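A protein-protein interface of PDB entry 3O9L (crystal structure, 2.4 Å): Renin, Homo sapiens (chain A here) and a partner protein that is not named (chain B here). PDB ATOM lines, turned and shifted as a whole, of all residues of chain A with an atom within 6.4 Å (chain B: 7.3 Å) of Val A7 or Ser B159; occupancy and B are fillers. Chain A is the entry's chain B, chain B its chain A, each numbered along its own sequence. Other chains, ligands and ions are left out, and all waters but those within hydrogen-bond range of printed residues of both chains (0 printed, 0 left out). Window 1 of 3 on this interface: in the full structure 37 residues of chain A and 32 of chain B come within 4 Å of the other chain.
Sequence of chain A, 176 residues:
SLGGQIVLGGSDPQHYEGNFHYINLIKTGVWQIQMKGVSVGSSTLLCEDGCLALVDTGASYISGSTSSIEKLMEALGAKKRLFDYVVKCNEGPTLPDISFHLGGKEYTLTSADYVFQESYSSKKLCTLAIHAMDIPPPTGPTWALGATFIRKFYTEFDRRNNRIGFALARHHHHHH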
ATOM      1  N   GLN A   5      -7.459  -2.589  12.421  1.00  0.00           N
ATOM      2  CA  GLN A   5      -8.385  -3.636  12.810  1.00  0.00           C
ATOM      3  C   GLN A   5      -8.055  -4.213  14.187  1.00  0.00           C
ATOM      4  O   GLN A   5      -6.875  -4.454  14.522  1.00  0.00           O
ATOM      5  CB  GLN A   5      -8.403  -4.745  11.752  1.00  0.00           C
ATOM      6  CG  GLN A   5      -9.379  -5.875  12.030  1.00  0.00           C
ATOM      7  CD  GLN A   5      -9.160  -7.060  11.130  1.00  0.00           C
ATOM      8  OE1 GLN A   5      -8.157  -7.761  11.250  1.00  0.00           O
ATOM      9  NE2 GLN A   5     -10.098  -7.303  10.228  1.00  0.00           N
ATOM     10  N   ILE A   6      -9.103  -4.446  14.977  1.00  0.00           N
ATOM     11  CA  ILE A   6      -8.948  -5.120  16.258  1.00  0.00           C
ATOM     12  C   ILE A   6      -9.803  -6.386  16.276  1.00  0.00           C
ATOM     13  O   ILE A   6     -11.010  -6.331  16.063  1.00  0.00           O
ATOM     14  CB  ILE A   6      -9.195  -4.154  17.469  1.00  0.00           C
ATOM     15  CG1 ILE A   6      -9.277  -4.929  18.785  1.00  0.00           C
ATOM     16  CG2 ILE A   6     -10.441  -3.314  17.256  1.00  0.00           C
ATOM     17  CD1 ILE A   6      -9.380  -4.058  20.049  1.00  0.00           C
ATOM     18  N   VAL A   7      -9.166  -7.531  16.502  1.00  0.00           N
ATOM     19  CA  VAL A   7      -9.881  -8.813  16.528  1.00  0.00           C
ATOM     20  C   VAL A   7     -10.047  -9.308  17.949  1.00  0.00           C
ATOM     21  O   VAL A   7      -9.083  -9.336  18.709  1.00  0.00           O
ATOM     22  CB  VAL A   7      -9.171  -9.890  15.673  1.00  0.00           C
ATOM     23  CG1 VAL A   7      -9.998 -11.175  15.623  1.00  0.00           C
ATOM     24  CG2 VAL A   7      -8.936  -9.369  14.263  1.00  0.00           C
ATOM     25  N   LEU A   8     -11.277  -9.679  18.311  1.00  0.00           N
ATOM     26  CA  LEU A   8     -11.549 -10.259  19.625  1.00  0.00           C
ATOM     27  C   LEU A   8     -11.717 -11.758  19.483  1.00  0.00           C
ATOM     28  O   LEU A   8     -12.632 -12.222  18.789  1.00  0.00           O
ATOM     29  CB  LEU A   8     -12.806  -9.666  20.265  1.00  0.00           C
ATOM     30  CG  LEU A   8     -13.007  -8.157  20.427  1.00  0.00           C
ATOM     31  CD1 LEU A   8     -14.497  -7.857  20.709  1.00  0.00           C
ATOM     32  CD2 LEU A   8     -12.130  -7.567  21.510  1.00  0.00           C
ATOM     33  N   GLY A   9     -10.813 -12.510  20.122  1.00  0.00           N
ATOM     34  CA  GLY A   9     -10.952 -13.959  20.196  1.00  0.00           C
ATOM     35  C   GLY A   9     -10.121 -14.728  19.194  1.00  0.00           C
ATOM     36  O   GLY A   9     -10.277 -15.945  19.051  1.00  0.00           O
ATOM     37  N   GLY A  10      -9.246 -14.012  18.504  1.00  0.00           N
ATOM     38  CA  GLY A  10      -8.292 -14.595  17.566  1.00  0.00           C
ATOM     39  C   GLY A  10      -7.382 -13.557  16.934  1.00  0.00           C
ATOM     40  O   GLY A  10      -7.256 -12.421  17.410  1.00  0.00           O
ATOM     41  N   SER A  11      -6.739 -13.949  15.851  1.00  0.00           N
ATOM     42  CA  SER A  11      -5.939 -13.023  15.067  1.00  0.00           C
ATOM     43  C   SER A  11      -6.400 -13.068  13.623  1.00  0.00           C
ATOM     44  O   SER A  11      -7.392 -13.737  13.304  1.00  0.00           O
ATOM     45  CB  SER A  11      -4.436 -13.320  15.204  1.00  0.00           C
ATOM     46  OG  SER A  11      -4.182 -14.610  15.739  1.00  0.00           O
ATOM     47  N   ASP A  12      -5.706 -12.338  12.752  1.00  0.00           N
ATOM     48  CA  ASP A  12      -6.026 -12.387  11.330  1.00  0.00           C
ATOM     49  C   ASP A  12      -4.756 -12.553  10.509  1.00  0.00           C
ATOM     50  O   ASP A  12      -3.970 -11.601  10.384  1.00  0.00           O
ATOM     51  CB  ASP A  12      -6.838 -11.167  10.889  1.00  0.00           C
ATOM     52  CG  ASP A  12      -7.499 -11.360   9.511  1.00  0.00           C
ATOM     53  OD1 ASP A  12      -7.477 -12.502   8.975  1.00  0.00           O
ATOM     54  OD2 ASP A  12      -8.039 -10.364   8.966  1.00  0.00           O
ATOM     55  N   PHE A  20       3.936 -16.237  15.725  1.00  0.00           N
ATOM     56  CA  PHE A  20       4.186 -15.287  16.809  1.00  0.00           C
ATOM     57  C   PHE A  20       5.364 -15.689  17.694  1.00  0.00           C
ATOM     58  O   PHE A  20       5.527 -16.862  18.056  1.00  0.00           O
ATOM     59  CB  PHE A  20       2.951 -15.089  17.710  1.00  0.00           C
ATOM     60  CG  PHE A  20       1.839 -14.303  17.070  1.00  0.00           C
ATOM     61  CD1 PHE A  20       1.909 -12.910  16.993  1.00  0.00           C
ATOM     62  CD2 PHE A  20       0.717 -14.953  16.557  1.00  0.00           C
ATOM     63  CE1 PHE A  20       0.909 -12.183  16.401  1.00  0.00           C
ATOM     64  CE2 PHE A  20      -0.309 -14.225  15.958  1.00  0.00           C
ATOM     65  CZ  PHE A  20      -0.207 -12.834  15.872  1.00  0.00           C
ATOM     66  N   TYR A 154       2.385  -6.676  14.235  1.00  0.00           N
ATOM     67  CA  TYR A 154       1.021  -7.102  14.574  1.00  0.00           C
ATOM     68  C   TYR A 154       1.026  -7.759  15.944  1.00  0.00           C
ATOM     69  O   TYR A 154       1.880  -8.567  16.231  1.00  0.00           O
ATOM     70  CB  TYR A 154       0.530  -8.082  13.504  1.00  0.00           C
ATOM     71  CG  TYR A 154      -0.881  -8.595  13.686  1.00  0.00           C
ATOM     72  CD1 TYR A 154      -1.154  -9.651  14.548  1.00  0.00           C
ATOM     73  CD2 TYR A 154      -1.924  -8.058  12.970  1.00  0.00           C
ATOM     74  CE1 TYR A 154      -2.442 -10.138  14.716  1.00  0.00           C
ATOM     75  CE2 TYR A 154      -3.225  -8.531  13.128  1.00  0.00           C
ATOM     76  CZ  TYR A 154      -3.473  -9.576  14.001  1.00  0.00           C
ATOM     77  OH  TYR A 154      -4.756 -10.058  14.149  1.00  0.00           O
ATOM     78  N   THR A 155       0.061  -7.428  16.791  1.00  0.00           N
ATOM     79  CA  THR A 155       0.176  -7.759  18.225  1.00  0.00           C
ATOM     80  C   THR A 155      -1.005  -8.523  18.827  1.00  0.00           C
ATOM     81  O   THR A 155      -2.141  -8.061  18.805  1.00  0.00           O
ATOM     82  CB  THR A 155       0.429  -6.487  19.060  1.00  0.00           C
ATOM     83  OG1 THR A 155       1.474  -5.702  18.454  1.00  0.00           O
ATOM     84  CG2 THR A 155       0.812  -6.860  20.482  1.00  0.00           C
ATOM     85  N   GLU A 156      -0.716  -9.683  19.404  1.00  0.00           N
ATOM     86  CA  GLU A 156      -1.729 -10.479  20.083  1.00  0.00           C
ATOM     87  C   GLU A 156      -1.564 -10.348  21.594  1.00  0.00           C
ATOM     88  O   GLU A 156      -0.456 -10.540  22.122  1.00  0.00           O
ATOM     89  CB  GLU A 156      -1.631 -11.940  19.648  1.00  0.00           C
ATOM     90  CG  GLU A 156      -2.817 -12.799  20.047  1.00  0.00           C
ATOM     91  CD  GLU A 156      -2.593 -14.275  19.752  1.00  0.00           C
ATOM     92  OE1 GLU A 156      -1.609 -14.836  20.283  1.00  0.00           O
ATOM     93  OE2 GLU A 156      -3.398 -14.878  19.006  1.00  0.00           O
ATOM     94  N   PHE A 157      -2.671  -9.996  22.266  1.00  0.00           N
ATOM     95  CA  PHE A 157      -2.746  -9.904  23.717  1.00  0.00           C
ATOM     96  C   PHE A 157      -3.527 -11.123  24.247  1.00  0.00           C
ATOM     97  O   PHE A 157      -4.745 -11.257  24.077  1.00  0.00           O
ATOM     98  CB  PHE A 157      -3.372  -8.567  24.165  1.00  0.00           C
ATOM     99  CG  PHE A 157      -2.635  -7.336  23.678  1.00  0.00           C
ATOM    100  CD1 PHE A 157      -1.580  -6.801  24.415  1.00  0.00           C
ATOM    101  CD2 PHE A 157      -2.978  -6.732  22.486  1.00  0.00           C
ATOM    102  CE1 PHE A 157      -0.890  -5.688  23.985  1.00  0.00           C
ATOM    103  CE2 PHE A 157      -2.291  -5.616  22.028  1.00  0.00           C
ATOM    104  CZ  PHE A 157      -1.235  -5.084  22.797  1.00  0.00           C
ATOM    105  N   THR B   7     -15.707 -15.067  16.411  1.00  0.00           N
ATOM    106  CA  THR B   7     -14.624 -14.097  16.345  1.00  0.00           C
ATOM    107  C   THR B   7     -15.245 -12.743  16.067  1.00  0.00           C
ATOM    108  O   THR B   7     -15.900 -12.551  15.035  1.00  0.00           O
ATOM    109  CB  THR B   7     -13.635 -14.388  15.196  1.00  0.00           C
ATOM    110  OG1 THR B   7     -14.357 -14.465  13.957  1.00  0.00           O
ATOM    111  CG2 THR B   7     -12.872 -15.685  15.437  1.00  0.00           C
ATOM    112  N   SER B   8     -15.047 -11.811  16.990  1.00  0.00           N
ATOM    113  CA  SER B   8     -15.465 -10.438  16.764  1.00  0.00           C
ATOM    114  C   SER B   8     -14.293  -9.656  16.199  1.00  0.00           C
ATOM    115  O   SER B   8     -13.147  -9.917  16.553  1.00  0.00           O
ATOM    116  CB  SER B   8     -15.938  -9.798  18.066  1.00  0.00           C
ATOM    117  OG  SER B   8     -16.377  -8.466  17.848  1.00  0.00           O
ATOM    118  N   SER B   9     -14.593  -8.703  15.322  1.00  0.00           N
ATOM    119  CA  SER B   9     -13.588  -7.817  14.748  1.00  0.00           C
ATOM    120  C   SER B   9     -14.176  -6.419  14.498  1.00  0.00           C
ATOM    121  O   SER B   9     -15.360  -6.287  14.189  1.00  0.00           O
ATOM    122  CB  SER B   9     -13.066  -8.401  13.437  1.00  0.00           C
ATOM    123  OG  SER B   9     -13.964  -8.109  12.382  1.00  0.00           O
ATOM    124  N   VAL B  10     -13.339  -5.388  14.623  1.00  0.00           N
ATOM    125  CA  VAL B  10     -13.781  -3.999  14.505  1.00  0.00           C
ATOM    126  C   VAL B  10     -12.813  -3.186  13.633  1.00  0.00           C
ATOM    127  O   VAL B  10     -11.607  -3.148  13.896  1.00  0.00           O
ATOM    128  CB  VAL B  10     -13.971  -3.336  15.921  1.00  0.00           C
ATOM    129  CG1 VAL B  10     -14.308  -1.842  15.811  1.00  0.00           C
ATOM    130  CG2 VAL B  10     -15.055  -4.078  16.761  1.00  0.00           C
ATOM    131  N   LEU B  12     -10.991   0.119  11.984  1.00  0.00           N
ATOM    132  CA  LEU B  12     -10.480   1.347  12.539  1.00  0.00           C
ATOM    133  C   LEU B  12     -10.280   2.412  11.495  1.00  0.00           C
ATOM    134  O   LEU B  12     -10.130   2.123  10.311  1.00  0.00           O
ATOM    135  CB  LEU B  12      -9.204   1.099  13.335  1.00  0.00           C
ATOM    136  CG  LEU B  12      -9.267  -0.013  14.401  1.00  0.00           C
ATOM    137  CD1 LEU B  12      -7.914  -0.246  15.073  1.00  0.00           C
ATOM    138  CD2 LEU B  12     -10.355   0.252  15.453  1.00  0.00           C
ATOM    139  N   MET B 130      -8.487  -1.812  27.721  1.00  0.00           N
ATOM    140  CA  MET B 130      -8.307  -3.258  27.500  1.00  0.00           C
ATOM    141  C   MET B 130      -7.392  -3.868  28.553  1.00  0.00           C
ATOM    142  O   MET B 130      -6.914  -4.999  28.402  1.00  0.00           O
ATOM    143  CB  MET B 130      -7.791  -3.569  26.093  1.00  0.00           C
ATOM    144  CG  MET B 130      -8.727  -3.142  24.954  1.00  0.00           C
ATOM    145  SD  MET B 130     -10.360  -3.933  24.956  1.00  0.00           S
ATOM    146  CE  MET B 130      -9.988  -5.585  24.359  1.00  0.00           C
ATOM    147  N   PHE B 144     -13.397  -6.573  28.591  1.00  0.00           N
ATOM    148  CA  PHE B 144     -12.919  -7.873  28.145  1.00  0.00           C
ATOM    149  C   PHE B 144     -13.087  -8.968  29.193  1.00  0.00           C
ATOM    150  O   PHE B 144     -13.182 -10.139  28.838  1.00  0.00           O
ATOM    151  CB  PHE B 144     -11.460  -7.818  27.646  1.00  0.00           C
ATOM    152  CG  PHE B 144     -11.119  -8.926  26.676  1.00  0.00           C
ATOM    153  CD1 PHE B 144     -11.726  -8.972  25.417  1.00  0.00           C
ATOM    154  CD2 PHE B 144     -10.232  -9.942  27.029  1.00  0.00           C
ATOM    155  CE1 PHE B 144     -11.440 -10.002  24.530  1.00  0.00           C
ATOM    156  CE2 PHE B 144      -9.938 -10.983  26.133  1.00  0.00           C
ATOM    157  CZ  PHE B 144     -10.547 -11.019  24.896  1.00  0.00           C
ATOM    158  N   VAL B 157      -8.097 -14.121  23.775  1.00  0.00           N
ATOM    159  CA  VAL B 157      -7.102 -13.220  23.208  1.00  0.00           C
ATOM    160  C   VAL B 157      -7.783 -12.134  22.363  1.00  0.00           C
ATOM    161  O   VAL B 157      -8.951 -12.260  21.989  1.00  0.00           O
ATOM    162  CB  VAL B 157      -6.056 -13.979  22.316  1.00  0.00           C
ATOM    163  CG1 VAL B 157      -5.505 -15.200  23.042  1.00  0.00           C
ATOM    164  CG2 VAL B 157      -6.672 -14.409  20.974  1.00  0.00           C
ATOM    165  N   PHE B 158      -7.043 -11.065  22.089  1.00  0.00           N
ATOM    166  CA  PHE B 158      -7.435 -10.042  21.117  1.00  0.00           C
ATOM    167  C   PHE B 158      -6.157  -9.475  20.473  1.00  0.00           C
ATOM    168  O   PHE B 158      -5.111  -9.405  21.126  1.00  0.00           O
ATOM    169  CB  PHE B 158      -8.301  -8.937  21.755  1.00  0.00           C
ATOM    170  CG  PHE B 158      -7.651  -8.251  22.913  1.00  0.00           C
ATOM    171  CD1 PHE B 158      -6.868  -7.103  22.714  1.00  0.00           C
ATOM    172  CD2 PHE B 158      -7.786  -8.763  24.198  1.00  0.00           C
ATOM    173  CE1 PHE B 158      -6.230  -6.467  23.796  1.00  0.00           C
ATOM    174  CE2 PHE B 158      -7.152  -8.135  25.287  1.00  0.00           C
ATOM    175  CZ  PHE B 158      -6.365  -6.984  25.083  1.00  0.00           C
ATOM    176  N   SER B 159      -6.264  -9.080  19.204  1.00  0.00           N
ATOM    177  CA  SER B 159      -5.127  -8.617  18.396  1.00  0.00           C
ATOM    178  C   SER B 159      -5.337  -7.256  17.750  1.00  0.00           C
ATOM    179  O   SER B 159      -6.474  -6.866  17.461  1.00  0.00           O
ATOM    180  CB  SER B 159      -4.835  -9.619  17.278  1.00  0.00           C
ATOM    181  OG  SER B 159      -4.796 -10.944  17.772  1.00  0.00           O
ATOM    182  N   PHE B 160      -4.226  -6.561  17.497  1.00  0.00           N
ATOM    183  CA  PHE B 160      -4.219  -5.265  16.805  1.00  0.00           C
ATOM    184  C   PHE B 160      -3.442  -5.221  15.485  1.00  0.00           C
ATOM    185  O   PHE B 160      -2.274  -5.589  15.429  1.00  0.00           O
ATOM    186  CB  PHE B 160      -3.641  -4.176  17.719  1.00  0.00           C
ATOM    187  CG  PHE B 160      -4.576  -3.722  18.812  1.00  0.00           C
ATOM    188  CD1 PHE B 160      -4.869  -4.555  19.884  1.00  0.00           C
ATOM    189  CD2 PHE B 160      -5.134  -2.452  18.779  1.00  0.00           C
ATOM    190  CE1 PHE B 160      -5.698  -4.134  20.907  1.00  0.00           C
ATOM    191  CE2 PHE B 160      -5.972  -2.020  19.795  1.00  0.00           C
ATOM    192  CZ  PHE B 160      -6.252  -2.868  20.864  1.00  0.00           C
ATOM    193  N   TYR B 161      -4.115  -4.723  14.445  1.00  0.00           N
ATOM    194  CA  TYR B 161      -3.502  -4.228  13.231  1.00  0.00           C
ATOM    195  C   TYR B 161      -3.784  -2.735  13.044  1.00  0.00           C
ATOM    196  O   TYR B 161      -4.961  -2.302  13.050  1.00  0.00           O
ATOM    197  CB  TYR B 161      -4.017  -5.004  12.010  1.00  0.00           C
ATOM    198  CG  TYR B 161      -3.639  -4.395  10.671  1.00  0.00           C
ATOM    199  CD1 TYR B 161      -2.300  -4.174  10.330  1.00  0.00           C
ATOM    200  CD2 TYR B 161      -4.621  -4.045   9.740  1.00  0.00           C
ATOM    201  CE1 TYR B 161      -1.946  -3.621   9.085  1.00  0.00           C
ATOM    202  CE2 TYR B 161      -4.278  -3.494   8.487  1.00  0.00           C
ATOM    203  CZ  TYR B 161      -2.934  -3.282   8.182  1.00  0.00           C
ATOM    204  OH  TYR B 161      -2.580  -2.727   6.972  1.00  0.00           O
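N of Gln A5 touches CD1 of Leu B12, 3.6 Å away. Ser B9 touches Ile A6 (CA to O, 3.3 Å). Ser B8 touches Val A7 (O to CA, 3.4 Å). N of Gly A10 touches CG2 of Val B157 (3.6 Å). Ser B159 touches Ser A11 (OG to CB, 3.5 Å). Tyr A154 touches Phe B160. OE2 of Glu A156 touches CG2 of Val B157 (3.8 Å). OG of Ser B159 touches CG of Glu A156, at 3.5 Å. Val B157 touches Phe A157. Phe A157 touches Phe B160 (CE2 to CD1, 3.5 Å).
Printed residues of chain B that touch a printed residue of chain A: Thr B7, Ser B8, Ser B9, Val B10, Leu B12, Phe B144, Val B157, Phe B158, Ser B159, Phe B160 and Tyr B161. Hydrophobic or aromatic side chains of chain B that line the printed part of chain A: Val B10, Leu B12, Phe B144, Val B157, Phe B158, Phe B160 and Tyr B161. Printed residues of chain A that touch a printed residue of chain B: Gln A5, Ile A6, Val A7, Leu A8, Gly A9, Gly A10, Ser A11, Tyr A154, Thr A155, Glu A156 and Phe A157. Hydrophobic or aromatic side chains of chain A within 4 Å of the printed part of chain B: Ile A6, Val A7, Leu A8, Tyr A154 and Phe A157. Among the printed residues, 32 pairs touch across the chains.
The side-chain amide oxygen (OE1) of Gln A5 sits close to the side-chain carboxylate (OD2) of Asp A12. The side-chain hydroxyl of Ser A11 is in hydrogen-bond range of the side-chain carboxylate of Glu A156, at 3.4 Å. OH of Tyr A154 is in hydrogen-bond range of N of Asp A12 (2.8 Å).
The backbone NH (N) of Val B10 is in hydrogen-bond range of the backbone carbonyl oxygen (O) of Ile A6 (2.9 Å). O of Phe B158 is in hydrogen-bond range of N of Phe A157 (2.8 Å). O of Val B157 is in hydrogen-bond range of N of Gly A9 (2.6 Å). The backbone carbonyl oxygen (O) of Gly A10 sits at hydrogen-bond distance from the side-chain hydroxyl (OG) of Ser B159 (2.9 Å). N of Gln A5 sits at hydrogen-bond distance from O of Tyr B161, 2.6 Å away. N of Leu A8 is in hydrogen-bond range of O of Ser B8 (2.6 Å). The backbone NH of Ser B159 is in hydrogen-bond range of the backbone carbonyl oxygen of Val A7 (2.9 Å). N of Phe B160 is in hydrogen-bond range of O of Thr A155, at 2.9 Å.
Printed residues of chain B within 4 Å of Gln A5: Val B10 (3.4 Å), Leu B12 (3.6 Å), Ser B159 (3.8 Å), Phe B160 (3.6 Å) and Tyr B161 (2.6 Å). Of the printed residues of chain B, Gly A9 touches Val B157 (2.6 Å). Printed residues of chain A within 4 Å of Leu B12: Gln A5 (3.6 Å) and Ile A6 (3.997 Å). Met B130 touches none of the printed residues of chain A. Of the printed residues of chain A, Phe B158 touches Val A7 (3.0 Å), Glu A156 (3.7 Å) and Phe A157 (2.8 Å). Ser B159 touches eight residues of chain A. Of the printed residues of chain A, Phe B160 touches Gln A5, Ile A6, Tyr A154, Thr A155 and Phe A157. The nearest residue of chain A that does not touch Ser B159 is Phe A157 (4.8 Å). The nearest printed residue of chain A that does not touch Ser B8 is Ile A6 (4.2 Å).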
